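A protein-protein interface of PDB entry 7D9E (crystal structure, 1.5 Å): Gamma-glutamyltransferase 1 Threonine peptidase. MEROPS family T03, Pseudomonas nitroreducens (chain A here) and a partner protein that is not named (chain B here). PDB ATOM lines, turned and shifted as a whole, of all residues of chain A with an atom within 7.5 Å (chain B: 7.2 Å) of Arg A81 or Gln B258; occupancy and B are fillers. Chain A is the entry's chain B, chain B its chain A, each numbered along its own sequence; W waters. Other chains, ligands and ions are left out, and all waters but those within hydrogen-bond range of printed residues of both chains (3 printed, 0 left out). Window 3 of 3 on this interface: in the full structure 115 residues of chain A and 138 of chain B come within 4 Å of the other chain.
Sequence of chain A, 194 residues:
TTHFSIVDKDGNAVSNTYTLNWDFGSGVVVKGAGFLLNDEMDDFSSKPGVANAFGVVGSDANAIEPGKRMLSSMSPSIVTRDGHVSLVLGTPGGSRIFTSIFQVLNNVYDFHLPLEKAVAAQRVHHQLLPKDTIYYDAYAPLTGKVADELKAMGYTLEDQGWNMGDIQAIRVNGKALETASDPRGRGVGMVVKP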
ATOM      1  N   VAL A  79       4.400  -6.872 -30.092  1.00  0.00           N
ATOM      2  CA  VAL A  79       5.817  -7.187 -30.124  1.00  0.00           C
ATOM      3  C   VAL A  79       5.982  -8.557 -30.757  1.00  0.00           C
ATOM      4  O   VAL A  79       5.227  -9.493 -30.450  1.00  0.00           O
ATOM      5  CB  VAL A  79       6.465  -7.184 -28.723  1.00  0.00           C
ATOM      6  CG1 VAL A  79       7.970  -7.327 -28.852  1.00  0.00           C
ATOM      7  CG2 VAL A  79       6.094  -5.930 -27.982  1.00  0.00           C
ATOM      8  N   THR A  80       6.980  -8.689 -31.617  1.00  0.00           N
ATOM      9  CA  THR A  80       7.326  -9.952 -32.248  1.00  0.00           C
ATOM     10  C   THR A  80       8.797 -10.258 -32.004  1.00  0.00           C
ATOM     11  O   THR A  80       9.596  -9.379 -31.663  1.00  0.00           O
ATOM     12  CB  THR A  80       7.039  -9.901 -33.758  1.00  0.00           C
ATOM     13  OG1 THR A  80       7.973  -9.025 -34.397  1.00  0.00           O
ATOM     14  CG2 THR A  80       5.638  -9.420 -34.011  1.00  0.00           C
ATOM     15  N   ARG A  81       9.146 -11.531 -32.187  1.00  0.00           N
ATOM     16  CA  ARG A  81      10.532 -11.976 -32.185  1.00  0.00           C
ATOM     17  C   ARG A  81      10.609 -13.130 -33.173  1.00  0.00           C
ATOM     18  O   ARG A  81       9.815 -14.069 -33.085  1.00  0.00           O
ATOM     19  CB  ARG A  81      10.954 -12.416 -30.781  1.00  0.00           C
ATOM     20  CG  ARG A  81      12.435 -12.641 -30.621  1.00  0.00           C
ATOM     21  CD  ARG A  81      12.804 -12.968 -29.184  1.00  0.00           C
ATOM     22  NE  ARG A  81      14.244 -13.143 -29.098  1.00  0.00           N
ATOM     23  CZ  ARG A  81      15.114 -12.182 -28.801  1.00  0.00           C
ATOM     24  NH1 ARG A  81      14.711 -10.960 -28.513  1.00  0.00           N
ATOM     25  NH2 ARG A  81      16.410 -12.463 -28.783  1.00  0.00           N
ATOM     26  N   ASP A  82      11.521 -13.029 -34.138  1.00  0.00           N
ATOM     27  CA  ASP A  82      11.717 -14.068 -35.153  1.00  0.00           C
ATOM     28  C   ASP A  82      10.471 -14.316 -35.996  1.00  0.00           C
ATOM     29  O   ASP A  82      10.211 -15.449 -36.417  1.00  0.00           O
ATOM     30  CB  ASP A  82      12.205 -15.380 -34.531  1.00  0.00           C
ATOM     31  CG  ASP A  82      13.443 -15.195 -33.682  1.00  0.00           C
ATOM     32  OD1 ASP A  82      14.267 -14.316 -34.009  1.00  0.00           O
ATOM     33  OD2 ASP A  82      13.579 -15.915 -32.676  1.00  0.00           O
ATOM     34  N   GLY A  83       9.690 -13.275 -36.262  1.00  0.00           N
ATOM     35  CA  GLY A  83       8.521 -13.424 -37.101  1.00  0.00           C
ATOM     36  C   GLY A  83       7.330 -14.049 -36.420  1.00  0.00           C
ATOM     37  O   GLY A  83       6.370 -14.442 -37.102  1.00  0.00           O
ATOM     38  N   HIS A  84       7.353 -14.152 -35.097  1.00  0.00           N
ATOM     39  CA  HIS A  84       6.226 -14.682 -34.353  1.00  0.00           C
ATOM     40  C   HIS A  84       5.841 -13.706 -33.260  1.00  0.00           C
ATOM     41  O   HIS A  84       6.698 -13.058 -32.655  1.00  0.00           O
ATOM     42  CB  HIS A  84       6.581 -16.030 -33.748  1.00  0.00           C
ATOM     43  CG  HIS A  84       6.959 -17.048 -34.772  1.00  0.00           C
ATOM     44  ND1 HIS A  84       8.268 -17.377 -35.046  1.00  0.00           N
ATOM     45  CD2 HIS A  84       6.199 -17.769 -35.629  1.00  0.00           C
ATOM     46  CE1 HIS A  84       8.299 -18.282 -36.008  1.00  0.00           C
ATOM     47  NE2 HIS A  84       7.058 -18.535 -36.382  1.00  0.00           N
ATOM     48  N   VAL A  85       4.536 -13.601 -33.027  1.00  0.00           N
ATOM     49  CA  VAL A  85       4.040 -12.732 -31.976  1.00  0.00           C
ATOM     50  C   VAL A  85       4.567 -13.209 -30.632  1.00  0.00           C
ATOM     51  O   VAL A  85       4.568 -14.406 -30.325  1.00  0.00           O
ATOM     52  CB  VAL A  85       2.506 -12.741 -32.005  1.00  0.00           C
ATOM     53  CG1 VAL A  85       1.943 -12.016 -30.805  1.00  0.00           C
ATOM     54  CG2 VAL A  85       2.009 -12.111 -33.297  1.00  0.00           C
ATOM     55  N   SER A  86       5.000 -12.256 -29.820  1.00  0.00           N
ATOM     56  CA  SER A  86       5.445 -12.529 -28.462  1.00  0.00           C
ATOM     57  C   SER A  86       4.644 -11.770 -27.416  1.00  0.00           C
ATOM     58  O   SER A  86       4.491 -12.285 -26.308  1.00  0.00           O
ATOM     59  CB  SER A  86       6.926 -12.183 -28.301  1.00  0.00           C
ATOM     60  OG  SER A  86       7.181 -10.844 -28.660  1.00  0.00           O
ATOM     61  N   LEU A  87       4.122 -10.580 -27.728  1.00  0.00           N
ATOM     62  CA  LEU A  87       3.370  -9.820 -26.740  1.00  0.00           C
ATOM     63  C   LEU A  87       2.395  -8.914 -27.460  1.00  0.00           C
ATOM     64  O   LEU A  87       2.772  -8.252 -28.427  1.00  0.00           O
ATOM     65  CB  LEU A  87       4.319  -8.985 -25.870  1.00  0.00           C
ATOM     66  CG  LEU A  87       3.682  -8.282 -24.661  1.00  0.00           C
ATOM     67  CD1 LEU A  87       3.260  -9.311 -23.624  1.00  0.00           C
ATOM     68  CD2 LEU A  87       4.655  -7.263 -24.069  1.00  0.00           C
ATOM     69  N   TYR A 109      10.621  -6.731 -20.221  1.00  0.00           N
ATOM     70  CA  TYR A 109      11.859  -6.956 -20.962  1.00  0.00           C
ATOM     71  C   TYR A 109      13.125  -6.576 -20.216  1.00  0.00           C
ATOM     72  O   TYR A 109      14.198  -7.104 -20.537  1.00  0.00           O
ATOM     73  CB  TYR A 109      11.807  -6.229 -22.319  1.00  0.00           C
ATOM     74  CG  TYR A 109      10.859  -6.896 -23.265  1.00  0.00           C
ATOM     75  CD1 TYR A 109      11.277  -7.992 -23.998  1.00  0.00           C
ATOM     76  CD2 TYR A 109       9.566  -6.457 -23.434  1.00  0.00           C
ATOM     77  CE1 TYR A 109      10.429  -8.642 -24.867  1.00  0.00           C
ATOM     78  CE2 TYR A 109       8.696  -7.113 -24.283  1.00  0.00           C
ATOM     79  CZ  TYR A 109       9.130  -8.190 -25.008  1.00  0.00           C
ATOM     80  OH  TYR A 109       8.324  -8.878 -25.864  1.00  0.00           O
ATOM     81  N   ASP A 110      13.050  -5.660 -19.263  1.00  0.00           N
ATOM     82  CA  ASP A 110      14.212  -5.278 -18.479  1.00  0.00           C
ATOM     83  C   ASP A 110      14.188  -5.840 -17.071  1.00  0.00           C
ATOM     84  O   ASP A 110      15.207  -6.327 -16.599  1.00  0.00           O
ATOM     85  CB  ASP A 110      14.336  -3.751 -18.428  1.00  0.00           C
ATOM     86  CG  ASP A 110      14.620  -3.147 -19.808  1.00  0.00           C
ATOM     87  OD1 ASP A 110      14.867  -3.911 -20.767  1.00  0.00           O
ATOM     88  OD2 ASP A 110      14.582  -1.904 -19.932  1.00  0.00           O
ATOM     89  N   TYR B  83      -1.153  -8.364 -36.816  1.00  0.00           N
ATOM     90  CA  TYR B  83      -0.097  -9.226 -37.330  1.00  0.00           C
ATOM     91  C   TYR B  83      -0.823 -10.436 -37.898  1.00  0.00           C
ATOM     92  O   TYR B  83      -1.345 -11.255 -37.141  1.00  0.00           O
ATOM     93  CB  TYR B  83       0.884  -9.599 -36.225  1.00  0.00           C
ATOM     94  CG  TYR B  83       2.240 -10.014 -36.704  1.00  0.00           C
ATOM     95  CD1 TYR B  83       3.116  -9.079 -37.234  1.00  0.00           C
ATOM     96  CD2 TYR B  83       2.676 -11.327 -36.575  1.00  0.00           C
ATOM     97  CE1 TYR B  83       4.371  -9.449 -37.662  1.00  0.00           C
ATOM     98  CE2 TYR B  83       3.934 -11.707 -36.995  1.00  0.00           C
ATOM     99  CZ  TYR B  83       4.787 -10.767 -37.522  1.00  0.00           C
ATOM    100  OH  TYR B  83       6.040 -11.157 -37.928  1.00  0.00           O
ATOM    101  N   ASP B 256      12.911  -1.551 -33.160  1.00  0.00           N
ATOM    102  CA  ASP B 256      13.691  -2.743 -32.872  1.00  0.00           C
ATOM    103  C   ASP B 256      14.590  -2.517 -31.667  1.00  0.00           C
ATOM    104  O   ASP B 256      15.273  -1.495 -31.580  1.00  0.00           O
ATOM    105  CB  ASP B 256      14.552  -3.079 -34.088  1.00  0.00           C
ATOM    106  CG  ASP B 256      13.743  -3.669 -35.229  1.00  0.00           C
ATOM    107  OD1 ASP B 256      13.562  -4.899 -35.263  1.00  0.00           O
ATOM    108  OD2 ASP B 256      13.274  -2.892 -36.076  1.00  0.00           O
ATOM    109  N   TRP B 257      14.618  -3.488 -30.757  1.00  0.00           N
ATOM    110  CA  TRP B 257      15.592  -3.424 -29.673  1.00  0.00           C
ATOM    111  C   TRP B 257      15.775  -4.831 -29.119  1.00  0.00           C
ATOM    112  O   TRP B 257      14.815  -5.603 -29.052  1.00  0.00           O
ATOM    113  CB  TRP B 257      15.114  -2.463 -28.565  1.00  0.00           C
ATOM    114  CG  TRP B 257      14.191  -3.045 -27.559  1.00  0.00           C
ATOM    115  CD1 TRP B 257      14.512  -3.353 -26.270  1.00  0.00           C
ATOM    116  CD2 TRP B 257      12.822  -3.430 -27.728  1.00  0.00           C
ATOM    117  NE1 TRP B 257      13.435  -3.883 -25.633  1.00  0.00           N
ATOM    118  CE2 TRP B 257      12.381  -3.946 -26.499  1.00  0.00           C
ATOM    119  CE3 TRP B 257      11.919  -3.370 -28.792  1.00  0.00           C
ATOM    120  CZ2 TRP B 257      11.085  -4.420 -26.305  1.00  0.00           C
ATOM    121  CZ3 TRP B 257      10.640  -3.847 -28.605  1.00  0.00           C
ATOM    122  CH2 TRP B 257      10.229  -4.363 -27.363  1.00  0.00           C
ATOM    123  N   GLN B 258      17.021  -5.160 -28.772  1.00  0.00           N
ATOM    124  CA  GLN B 258      17.349  -6.431 -28.110  1.00  0.00           C
ATOM    125  C   GLN B 258      16.782  -7.642 -28.857  1.00  0.00           C
ATOM    126  O   GLN B 258      16.414  -8.653 -28.248  1.00  0.00           O
ATOM    127  CB  GLN B 258      16.898  -6.434 -26.642  1.00  0.00           C
ATOM    128  CG  GLN B 258      17.596  -5.396 -25.764  1.00  0.00           C
ATOM    129  CD  GLN B 258      19.087  -5.650 -25.626  1.00  0.00           C
ATOM    130  N   GLY B 259      16.727  -7.567 -30.185  1.00  0.00           N
ATOM    131  CA  GLY B 259      16.222  -8.658 -30.990  1.00  0.00           C
ATOM    132  C   GLY B 259      14.717  -8.727 -31.115  1.00  0.00           C
ATOM    133  O   GLY B 259      14.211  -9.621 -31.804  1.00  0.00           O
ATOM    134  N   ASN B 260      13.988  -7.837 -30.457  1.00  0.00           N
ATOM    135  CA  ASN B 260      12.537  -7.765 -30.554  1.00  0.00           C
ATOM    136  C   ASN B 260      12.129  -6.684 -31.542  1.00  0.00           C
ATOM    137  O   ASN B 260      12.858  -5.714 -31.758  1.00  0.00           O
ATOM    138  CB  ASN B 260      11.926  -7.417 -29.201  1.00  0.00           C
ATOM    139  CG  ASN B 260      12.431  -8.277 -28.100  1.00  0.00           C
ATOM    140  OD1 ASN B 260      12.121  -9.469 -28.045  1.00  0.00           O
ATOM    141  ND2 ASN B 260      13.267  -7.703 -27.236  1.00  0.00           N
ATOM    142  N   THR B 261      10.954  -6.863 -32.140  1.00  0.00           N
ATOM    143  CA  THR B 261      10.394  -5.879 -33.054  1.00  0.00           C
ATOM    144  C   THR B 261       9.013  -5.489 -32.551  1.00  0.00           C
ATOM    145  O   THR B 261       8.115  -6.336 -32.493  1.00  0.00           O
ATOM    146  CB  THR B 261      10.296  -6.429 -34.478  1.00  0.00           C
ATOM    147  OG1 THR B 261      11.606  -6.815 -34.911  1.00  0.00           O
ATOM    148  CG2 THR B 261       9.715  -5.364 -35.403  1.00  0.00           C
ATOM    149  N   GLU B 283      17.564   2.749 -23.826  1.00  0.00           N
ATOM    150  CA  GLU B 283      18.675   1.882 -24.210  1.00  0.00           C
ATOM    151  C   GLU B 283      19.995   2.646 -24.208  1.00  0.00           C
ATOM    152  O   GLU B 283      21.022   2.128 -23.755  1.00  0.00           O
ATOM    153  CB  GLU B 283      18.418   1.246 -25.575  1.00  0.00           C
ATOM    154  CG  GLU B 283      17.226   0.282 -25.610  1.00  0.00           C
ATOM    155  CD  GLU B 283      17.526  -1.109 -25.065  1.00  0.00           C
ATOM    156  OE1 GLU B 283      18.122  -1.932 -25.798  1.00  0.00           O
ATOM    157  OE2 GLU B 283      17.128  -1.393 -23.916  1.00  0.00           O
HETATM  158  O   HOH W   1      12.486  -9.712 -34.155  1.00  0.00           O
HETATM  159  O   HOH W   2       9.647 -10.559 -27.521  1.00  0.00           O
HETATM  160  O   HOH W   3      18.732 -10.835 -28.024  1.00  0.00           O
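O of Gly A83 sits at hydrogen-bond distance from OH of Tyr B83, at 3.4 Å.
O of Gln B258 is in hydrogen-bond range of NH1 of Arg A81.
NH1 of Arg A81 sits at hydrogen-bond distance from OD1 of Asn B260, at 3.0 Å.
The backbone carbonyl oxygen of Thr B261 is in hydrogen-bond range of the backbone NH of Thr A80 (2.8 Å).
Water W2 lies within hydrogen-bond range of OH of Tyr A109 (2.7 Å), OG of Ser A86 (2.7 Å) and OD1 of Asn B260 (2.8 Å).
Water W1 lies within hydrogen-bond range of the backbone carbonyl oxygen (O) of Gly B259, the side-chain hydroxyl (OG1) of Thr B261 and the backbone NH (N) of Asp A82.
Water W3 lies within hydrogen-bond range of NH2 of Arg A81 (2.9 Å) and O of Gln B258 (3.2 Å).
Printed residues of chain B within 4 Å of Val A79: Asn B260 (3.97 Å) and Thr B261 (3.4 Å).
Of chain B, only Gln B258, Gly B259 and Asn B260 come within 4 Å of Arg A81.
Of the printed residues of chain B, Val A85 touches Tyr B83.
Of the printed residues of chain A, Tyr B83 touches Thr A80 (3.9 Å), Gly A83 (3.4 Å) and Val A85 (3.4 Å).
Printed residues of chain A within 4 Å of Thr B261: Val A79 (3.4 Å) and Thr A80 (2.8 Å).
The nearest residue of chain B that does not touch Arg A81 is Thr B261 (5.0 Å).
The nearest residue of chain A that does not touch Gln B258 is Asp A110 (5.9 Å).
The side-chain carboxylate (OD1) of Asp B256 lies within hydrogen-bond range of the side-chain hydroxyl (OG1) of Thr B261, 2.8 Å away.
The backbone carbonyl oxygen (O) of Trp B257 is in hydrogen-bond range of the side-chain amide nitrogen (ND2) of Asn B260, 3.2 Å away.
O of Gln B258 sits at hydrogen-bond distance from ND2 of Asn B260 (3.4 Å).
O of Val A79 sits at hydrogen-bond distance from N of Ser A86 (2.8 Å).
N of Val A79 sits at hydrogen-bond distance from O of Leu A87.
Printed residues of chain A that touch a printed residue of chain B: Val A79, Thr A80, Arg A81, Gly A83, Val A85 and Tyr A109.
Hydrophobic or aromatic side chains of chain A that line the printed part of chain B: Val A79, Val A85 and Tyr A109.
Of the 8 printed residues of chain B, 6 touch a printed residue of chain A.
Printed residues of chain B that touch a printed residue of chain A: Tyr B83, Trp B257, Gln B258, Gly B259, Asn B260 and Thr B261.
Val A79 touches Asn B260 (CG1 to CB, 3.97 Å).
Val A79 touches Thr B261.
Tyr B83 touches Thr A80.
O of Thr A80 touches CA of Asn B260 (3.5 Å).
Gly B259 touches Arg A81.
CD2 of Tyr B83 touches CG2 of Val A85, 3.4 Å away.
Tyr A109 touches Trp B257 (CD2 to CZ2, 3.8 Å).
CE1 of Tyr A109 touches OD1 of Asn B260, at 3.7 Å.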
